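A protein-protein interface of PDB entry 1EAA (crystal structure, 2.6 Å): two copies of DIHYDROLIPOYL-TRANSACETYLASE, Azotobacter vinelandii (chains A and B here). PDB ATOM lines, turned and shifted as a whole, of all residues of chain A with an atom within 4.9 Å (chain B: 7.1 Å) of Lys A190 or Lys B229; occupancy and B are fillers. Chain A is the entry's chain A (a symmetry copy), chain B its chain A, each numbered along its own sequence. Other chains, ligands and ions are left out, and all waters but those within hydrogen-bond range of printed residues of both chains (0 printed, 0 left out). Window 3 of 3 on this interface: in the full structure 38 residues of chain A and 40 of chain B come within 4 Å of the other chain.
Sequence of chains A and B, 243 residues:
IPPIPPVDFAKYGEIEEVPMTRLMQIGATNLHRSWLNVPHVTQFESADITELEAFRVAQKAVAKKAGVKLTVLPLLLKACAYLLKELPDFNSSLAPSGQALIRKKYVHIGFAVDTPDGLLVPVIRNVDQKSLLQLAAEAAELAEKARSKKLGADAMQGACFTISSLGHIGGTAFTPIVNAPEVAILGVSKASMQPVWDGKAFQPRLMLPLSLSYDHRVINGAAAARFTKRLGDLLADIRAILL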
ATOM      1  N   GLY A 167     -20.246  -3.668  24.871  1.00  0.00           N
ATOM      2  CA  GLY A 167     -21.150  -3.014  25.770  1.00  0.00           C
ATOM      3  C   GLY A 167     -22.490  -2.775  25.113  1.00  0.00           C
ATOM      4  O   GLY A 167     -23.542  -2.789  25.744  1.00  0.00           O
ATOM      5  N   ILE A 169     -24.197  -4.820  23.223  1.00  0.00           N
ATOM      6  CA  ILE A 169     -25.018  -5.981  22.958  1.00  0.00           C
ATOM      7  C   ILE A 169     -25.291  -6.461  24.356  1.00  0.00           C
ATOM      8  O   ILE A 169     -26.467  -6.668  24.642  1.00  0.00           O
ATOM      9  CB  ILE A 169     -24.242  -7.000  22.137  1.00  0.00           C
ATOM     10  CG1 ILE A 169     -23.861  -6.398  20.826  1.00  0.00           C
ATOM     11  CG2 ILE A 169     -25.109  -8.184  21.793  1.00  0.00           C
ATOM     12  CD1 ILE A 169     -22.726  -7.187  20.237  1.00  0.00           C
ATOM     13  N   GLY A 170     -24.325  -6.611  25.261  1.00  0.00           N
ATOM     14  CA  GLY A 170     -24.704  -7.035  26.574  1.00  0.00           C
ATOM     15  C   GLY A 170     -23.582  -7.811  27.166  1.00  0.00           C
ATOM     16  O   GLY A 170     -22.460  -7.802  26.662  1.00  0.00           O
ATOM     17  N   GLY A 171     -23.864  -8.505  28.247  1.00  0.00           N
ATOM     18  CA  GLY A 171     -22.858  -9.311  28.891  1.00  0.00           C
ATOM     19  C   GLY A 171     -22.290  -8.566  30.083  1.00  0.00           C
ATOM     20  O   GLY A 171     -22.280  -7.348  30.268  1.00  0.00           O
ATOM     21  N   VAL A 188     -14.590  -4.781  27.042  1.00  0.00           N
ATOM     22  CA  VAL A 188     -15.490  -3.891  27.755  1.00  0.00           C
ATOM     23  C   VAL A 188     -16.905  -4.404  27.542  1.00  0.00           C
ATOM     24  O   VAL A 188     -17.310  -4.672  26.396  1.00  0.00           O
ATOM     25  CB  VAL A 188     -15.468  -2.439  27.219  1.00  0.00           C
ATOM     26  CG1 VAL A 188     -16.376  -1.580  28.043  1.00  0.00           C
ATOM     27  CG2 VAL A 188     -14.104  -1.833  27.382  1.00  0.00           C
ATOM     28  N   SER A 189     -17.690  -4.486  28.602  1.00  0.00           N
ATOM     29  CA  SER A 189     -19.059  -4.954  28.517  1.00  0.00           C
ATOM     30  C   SER A 189     -20.158  -3.942  28.891  1.00  0.00           C
ATOM     31  O   SER A 189     -19.937  -2.726  28.836  1.00  0.00           O
ATOM     32  CB  SER A 189     -19.111  -6.237  29.350  1.00  0.00           C
ATOM     33  OG  SER A 189     -18.319  -7.298  28.810  1.00  0.00           O
ATOM     34  N   LYS A 190     -21.362  -4.360  29.225  1.00  0.00           N
ATOM     35  CA  LYS A 190     -22.485  -3.490  29.436  1.00  0.00           C
ATOM     36  C   LYS A 190     -22.393  -2.885  30.796  1.00  0.00           C
ATOM     37  O   LYS A 190     -22.151  -3.630  31.745  1.00  0.00           O
ATOM     38  CB  LYS A 190     -23.768  -4.239  29.379  1.00  0.00           C
ATOM     39  CG  LYS A 190     -24.756  -3.425  28.657  1.00  0.00           C
ATOM     40  CD  LYS A 190     -26.169  -3.685  29.172  1.00  0.00           C
ATOM     41  CE  LYS A 190     -27.206  -3.009  28.222  1.00  0.00           C
ATOM     42  NZ  LYS A 190     -27.486  -3.768  26.990  1.00  0.00           N
ATOM     43  N   ALA A 191     -22.638  -1.569  30.843  1.00  0.00           N
ATOM     44  CA  ALA A 191     -22.610  -0.818  32.094  1.00  0.00           C
ATOM     45  C   ALA A 191     -23.927  -1.049  32.772  1.00  0.00           C
ATOM     46  O   ALA A 191     -24.940  -1.137  32.064  1.00  0.00           O
ATOM     47  CB  ALA A 191     -22.528   0.625  31.820  1.00  0.00           C
ATOM     48  N   SER A 192     -23.952  -1.127  34.106  1.00  0.00           N
ATOM     49  CA  SER A 192     -25.189  -1.310  34.835  1.00  0.00           C
ATOM     50  C   SER A 192     -25.119  -0.479  36.092  1.00  0.00           C
ATOM     51  O   SER A 192     -24.029  -0.170  36.589  1.00  0.00           O
ATOM     52  CB  SER A 192     -25.390  -2.679  35.328  1.00  0.00           C
ATOM     53  OG  SER A 192     -24.974  -3.634  34.405  1.00  0.00           O
ATOM     54  N   MET A 207     -21.547   1.367  36.571  1.00  0.00           N
ATOM     55  CA  MET A 207     -20.275   0.667  36.590  1.00  0.00           C
ATOM     56  C   MET A 207     -20.013  -0.014  35.270  1.00  0.00           C
ATOM     57  O   MET A 207     -20.840  -0.798  34.813  1.00  0.00           O
ATOM     58  CB  MET A 207     -20.355  -0.335  37.685  1.00  0.00           C
ATOM     59  CG  MET A 207     -20.490   0.279  39.047  1.00  0.00           C
ATOM     60  SD  MET A 207     -18.880   0.705  39.776  1.00  0.00           S
ATOM     61  CE  MET A 207     -19.438   2.316  39.995  1.00  0.00           C
ATOM     62  N   PRO A 209     -18.014  -2.797  33.191  1.00  0.00           N
ATOM     63  CA  PRO A 209     -17.182  -3.990  33.439  1.00  0.00           C
ATOM     64  C   PRO A 209     -15.963  -4.049  32.532  1.00  0.00           C
ATOM     65  O   PRO A 209     -16.113  -3.801  31.345  1.00  0.00           O
ATOM     66  CB  PRO A 209     -18.147  -5.119  33.236  1.00  0.00           C
ATOM     67  CG  PRO A 209     -19.515  -4.446  33.335  1.00  0.00           C
ATOM     68  CD  PRO A 209     -19.293  -3.135  32.613  1.00  0.00           C
ATOM     69  N   GLN B  43     -18.074 -15.930  27.723  1.00  0.00           N
ATOM     70  CA  GLN B  43     -18.942 -14.797  27.860  1.00  0.00           C
ATOM     71  C   GLN B  43     -19.799 -14.983  29.112  1.00  0.00           C
ATOM     72  O   GLN B  43     -20.508 -15.964  29.273  1.00  0.00           O
ATOM     73  CB  GLN B  43     -19.772 -14.709  26.594  1.00  0.00           C
ATOM     74  CG  GLN B  43     -20.861 -13.652  26.638  1.00  0.00           C
ATOM     75  CD  GLN B  43     -20.372 -12.236  26.602  1.00  0.00           C
ATOM     76  OE1 GLN B  43     -19.663 -11.853  25.685  1.00  0.00           O
ATOM     77  NE2 GLN B  43     -20.700 -11.401  27.560  1.00  0.00           N
ATOM     78  N   GLU B  45     -22.889 -13.631  31.641  1.00  0.00           N
ATOM     79  CA  GLU B  45     -24.169 -12.928  31.622  1.00  0.00           C
ATOM     80  C   GLU B  45     -24.937 -13.430  32.849  1.00  0.00           C
ATOM     81  O   GLU B  45     -24.502 -14.468  33.396  1.00  0.00           O
ATOM     82  CB  GLU B  45     -25.030 -13.264  30.403  1.00  0.00           C
ATOM     83  CG  GLU B  45     -26.337 -12.458  30.269  1.00  0.00           C
ATOM     84  CD  GLU B  45     -26.203 -10.932  30.442  1.00  0.00           C
ATOM     85  OE1 GLU B  45     -26.041 -10.432  31.580  1.00  0.00           O
ATOM     86  OE2 GLU B  45     -26.251 -10.229  29.430  1.00  0.00           O
ATOM     87  N   LEU B  83     -33.284 -21.178  21.040  1.00  0.00           N
ATOM     88  CA  LEU B  83     -32.230 -20.276  20.637  1.00  0.00           C
ATOM     89  C   LEU B  83     -31.262 -20.860  19.667  1.00  0.00           C
ATOM     90  O   LEU B  83     -30.808 -20.163  18.790  1.00  0.00           O
ATOM     91  CB  LEU B  83     -31.437 -19.789  21.840  1.00  0.00           C
ATOM     92  CG  LEU B  83     -31.628 -18.349  22.294  1.00  0.00           C
ATOM     93  CD1 LEU B  83     -30.641 -18.081  23.411  1.00  0.00           C
ATOM     94  CD2 LEU B  83     -31.392 -17.376  21.150  1.00  0.00           C
ATOM     95  N   LEU B 210     -24.539 -17.225  34.151  1.00  0.00           N
ATOM     96  CA  LEU B 210     -24.402 -18.115  32.998  1.00  0.00           C
ATOM     97  C   LEU B 210     -23.013 -17.896  32.444  1.00  0.00           C
ATOM     98  O   LEU B 210     -22.532 -16.768  32.548  1.00  0.00           O
ATOM     99  CB  LEU B 210     -25.392 -17.756  31.954  1.00  0.00           C
ATOM    100  CG  LEU B 210     -26.886 -17.761  32.319  1.00  0.00           C
ATOM    101  CD1 LEU B 210     -27.586 -16.916  31.276  1.00  0.00           C
ATOM    102  CD2 LEU B 210     -27.423 -19.203  32.476  1.00  0.00           C
ATOM    103  N   ALA B 223     -21.513 -12.244  18.390  1.00  0.00           N
ATOM    104  CA  ALA B 223     -22.524 -13.279  18.233  1.00  0.00           C
ATOM    105  C   ALA B 223     -22.753 -13.919  19.570  1.00  0.00           C
ATOM    106  O   ALA B 223     -23.896 -14.135  19.968  1.00  0.00           O
ATOM    107  CB  ALA B 223     -22.070 -14.359  17.306  1.00  0.00           C
ATOM    108  N   ALA B 224     -21.695 -14.183  20.330  1.00  0.00           N
ATOM    109  CA  ALA B 224     -21.876 -14.775  21.637  1.00  0.00           C
ATOM    110  C   ALA B 224     -22.566 -13.865  22.633  1.00  0.00           C
ATOM    111  O   ALA B 224     -23.279 -14.420  23.471  1.00  0.00           O
ATOM    112  CB  ALA B 224     -20.576 -15.131  22.234  1.00  0.00           C
ATOM    113  N   ALA B 225     -22.384 -12.527  22.623  1.00  0.00           N
ATOM    114  CA  ALA B 225     -23.048 -11.660  23.606  1.00  0.00           C
ATOM    115  C   ALA B 225     -24.515 -11.542  23.308  1.00  0.00           C
ATOM    116  O   ALA B 225     -25.319 -11.378  24.217  1.00  0.00           O
ATOM    117  CB  ALA B 225     -22.521 -10.242  23.626  1.00  0.00           C
ATOM    118  N   ARG B 226     -24.865 -11.620  22.019  1.00  0.00           N
ATOM    119  CA  ARG B 226     -26.224 -11.654  21.524  1.00  0.00           C
ATOM    120  C   ARG B 226     -26.805 -12.998  21.953  1.00  0.00           C
ATOM    121  O   ARG B 226     -27.942 -13.022  22.430  1.00  0.00           O
ATOM    122  CB  ARG B 226     -26.086 -11.494  20.065  1.00  0.00           C
ATOM    123  CG  ARG B 226     -27.280 -11.047  19.258  1.00  0.00           C
ATOM    124  CD  ARG B 226     -26.814 -10.612  17.825  1.00  0.00           C
ATOM    125  NE  ARG B 226     -25.906  -9.448  17.783  1.00  0.00           N
ATOM    126  CZ  ARG B 226     -26.295  -8.146  17.965  1.00  0.00           C
ATOM    127  NH1 ARG B 226     -27.564  -7.739  18.201  1.00  0.00           N
ATOM    128  NH2 ARG B 226     -25.357  -7.189  17.971  1.00  0.00           N
ATOM    129  N   PHE B 227     -26.129 -14.148  21.900  1.00  0.00           N
ATOM    130  CA  PHE B 227     -26.722 -15.377  22.402  1.00  0.00           C
ATOM    131  C   PHE B 227     -26.971 -15.319  23.893  1.00  0.00           C
ATOM    132  O   PHE B 227     -28.075 -15.735  24.261  1.00  0.00           O
ATOM    133  CB  PHE B 227     -25.836 -16.548  22.155  1.00  0.00           C
ATOM    134  CG  PHE B 227     -26.342 -17.928  22.508  1.00  0.00           C
ATOM    135  CD1 PHE B 227     -26.202 -18.411  23.788  1.00  0.00           C
ATOM    136  CD2 PHE B 227     -26.896 -18.718  21.524  1.00  0.00           C
ATOM    137  CE1 PHE B 227     -26.618 -19.708  24.064  1.00  0.00           C
ATOM    138  CE2 PHE B 227     -27.302 -20.007  21.811  1.00  0.00           C
ATOM    139  CZ  PHE B 227     -27.166 -20.514  23.083  1.00  0.00           C
ATOM    140  N   THR B 228     -26.069 -14.901  24.808  1.00  0.00           N
ATOM    141  CA  THR B 228     -26.418 -14.924  26.221  1.00  0.00           C
ATOM    142  C   THR B 228     -27.424 -13.830  26.554  1.00  0.00           C
ATOM    143  O   THR B 228     -28.208 -13.956  27.497  1.00  0.00           O
ATOM    144  CB  THR B 228     -25.171 -14.766  27.122  1.00  0.00           C
ATOM    145  OG1 THR B 228     -24.431 -13.662  26.630  1.00  0.00           O
ATOM    146  CG2 THR B 228     -24.286 -15.978  27.144  1.00  0.00           C
ATOM    147  N   LYS B 229     -27.478 -12.738  25.798  1.00  0.00           N
ATOM    148  CA  LYS B 229     -28.484 -11.711  26.029  1.00  0.00           C
ATOM    149  C   LYS B 229     -29.850 -12.280  25.696  1.00  0.00           C
ATOM    150  O   LYS B 229     -30.752 -12.190  26.518  1.00  0.00           O
ATOM    151  CB  LYS B 229     -28.240 -10.476  25.150  1.00  0.00           C
ATOM    152  CG  LYS B 229     -28.993  -9.279  25.634  1.00  0.00           C
ATOM    153  CD  LYS B 229     -29.951  -8.791  24.583  1.00  0.00           C
ATOM    154  CE  LYS B 229     -30.655  -7.539  25.147  1.00  0.00           C
ATOM    155  NZ  LYS B 229     -29.729  -6.438  25.496  1.00  0.00           N
ATOM    156  N   ARG B 230     -30.016 -12.893  24.522  1.00  0.00           N
ATOM    157  CA  ARG B 230     -31.275 -13.485  24.133  1.00  0.00           C
ATOM    158  C   ARG B 230     -31.641 -14.514  25.154  1.00  0.00           C
ATOM    159  O   ARG B 230     -32.783 -14.503  25.574  1.00  0.00           O
ATOM    160  CB  ARG B 230     -31.184 -14.175  22.794  1.00  0.00           C
ATOM    161  CG  ARG B 230     -31.323 -13.284  21.577  1.00  0.00           C
ATOM    162  CD  ARG B 230     -32.742 -12.776  21.652  1.00  0.00           C
ATOM    163  NE  ARG B 230     -33.809 -13.628  21.121  1.00  0.00           N
ATOM    164  CZ  ARG B 230     -35.003 -13.763  21.710  1.00  0.00           C
ATOM    165  NH1 ARG B 230     -35.352 -13.204  22.870  1.00  0.00           N
ATOM    166  NH2 ARG B 230     -35.992 -14.266  20.994  1.00  0.00           N
ATOM    167  N   LEU B 231     -30.719 -15.362  25.599  1.00  0.00           N
ATOM    168  CA  LEU B 231     -30.994 -16.404  26.585  1.00  0.00           C
ATOM    169  C   LEU B 231     -31.441 -15.792  27.895  1.00  0.00           C
ATOM    170  O   LEU B 231     -32.382 -16.265  28.524  1.00  0.00           O
ATOM    171  CB  LEU B 231     -29.740 -17.260  26.821  1.00  0.00           C
ATOM    172  CG  LEU B 231     -29.804 -18.325  27.865  1.00  0.00           C
ATOM    173  CD1 LEU B 231     -30.786 -19.381  27.461  1.00  0.00           C
ATOM    174  CD2 LEU B 231     -28.486 -19.012  27.961  1.00  0.00           C
ATOM    175  N   GLY B 232     -30.828 -14.704  28.321  1.00  0.00           N
ATOM    176  CA  GLY B 232     -31.215 -14.019  29.536  1.00  0.00           C
ATOM    177  C   GLY B 232     -32.631 -13.553  29.379  1.00  0.00           C
ATOM    178  O   GLY B 232     -33.387 -13.649  30.331  1.00  0.00           O
ATOM    179  N   ASP B 233     -33.031 -13.119  28.176  1.00  0.00           N
ATOM    180  CA  ASP B 233     -34.354 -12.591  27.861  1.00  0.00           C
ATOM    181  C   ASP B 233     -35.321 -13.743  27.880  1.00  0.00           C
ATOM    182  O   ASP B 233     -36.367 -13.640  28.495  1.00  0.00           O
ATOM    183  CB  ASP B 233     -34.478 -11.960  26.461  1.00  0.00           C
ATOM    184  CG  ASP B 233     -33.818 -10.603  26.147  1.00  0.00           C
ATOM    185  OD1 ASP B 233     -33.422  -9.894  27.075  1.00  0.00           O
ATOM    186  OD2 ASP B 233     -33.712 -10.248  24.952  1.00  0.00           O
ATOM    187  N   LEU B 234     -35.016 -14.856  27.246  1.00  0.00           N
ATOM    188  CA  LEU B 234     -35.905 -15.986  27.265  1.00  0.00           C
ATOM    189  C   LEU B 234     -36.092 -16.513  28.662  1.00  0.00           C
ATOM    190  O   LEU B 234     -37.217 -16.844  28.967  1.00  0.00           O
ATOM    191  CB  LEU B 234     -35.373 -17.107  26.406  1.00  0.00           C
ATOM    192  CG  LEU B 234     -35.312 -16.844  24.935  1.00  0.00           C
ATOM    193  CD1 LEU B 234     -34.596 -17.983  24.336  1.00  0.00           C
ATOM    194  CD2 LEU B 234     -36.671 -16.744  24.313  1.00  0.00           C
ATOM    195  N   LEU B 235     -35.099 -16.640  29.537  1.00  0.00           N
ATOM    196  CA  LEU B 235     -35.309 -17.155  30.881  1.00  0.00           C
ATOM    197  C   LEU B 235     -36.112 -16.187  31.774  1.00  0.00           C
ATOM    198  O   LEU B 235     -36.822 -16.591  32.697  1.00  0.00           O
ATOM    199  CB  LEU B 235     -33.930 -17.455  31.502  1.00  0.00           C
ATOM    200  CG  LEU B 235     -33.070 -18.578  30.951  1.00  0.00           C
ATOM    201  CD1 LEU B 235     -31.880 -18.765  31.860  1.00  0.00           C
ATOM    202  CD2 LEU B 235     -33.805 -19.889  30.971  1.00  0.00           C
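The side-chain carboxylate (OE2) of Glu B45 lies within hydrogen-bond range of the backbone NH (N) of Gly A171 (3.2 Å). O of Ile A169 sits at hydrogen-bond distance from NZ of Lys B229 (3.4 Å).
Ala B225 touches Ile A169. CG1 of Ile A169 touches NH2 of Arg B226, at 3.3 Å. O of Gly A170 touches CB of Ala B225, at 3.9 Å. Gln B43 touches Gly A171. NZ of Lys B229 touches NZ of Lys A190, at 3.8 Å.
The backbone carbonyl oxygen of Ala B225 lies within hydrogen-bond range of the side-chain hydroxyl of Thr B228. O of Gly A171 sits at hydrogen-bond distance from N of Lys A190 (3.3 Å). O of Glu B45 is in hydrogen-bond range of N of Leu B210 (2.9 Å).
Of the printed residues of chain B, Gly A170 touches Ala B225 (3.9 Å). Of chain B, only Lys B229 (3.8 Å) comes within 4 Å of Lys A190. Met A207 touches none of the printed residues of chain B. Printed residues of chain A within 4 Å of Ala B225: Ile A169 (3.7 Å) and Gly A170 (3.9 Å). Of the printed residues of chain A, Arg B226 touches Ile A169 (3.3 Å). Lys B229 touches two residues of chain A. The nearest printed residue of chain A that does not touch Lys B229 is Gly A170 (4.9 Å).
Of the 17 printed residues of chain B, 5 touch a printed residue of chain A. Among the printed residues, 7 pairs touch across the chains. Among the printed residues, no Asp or Glu carboxylate lies within 4 Å of a Lys or Arg side-chain nitrogen of the other chain.
No position is printed for both chains.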
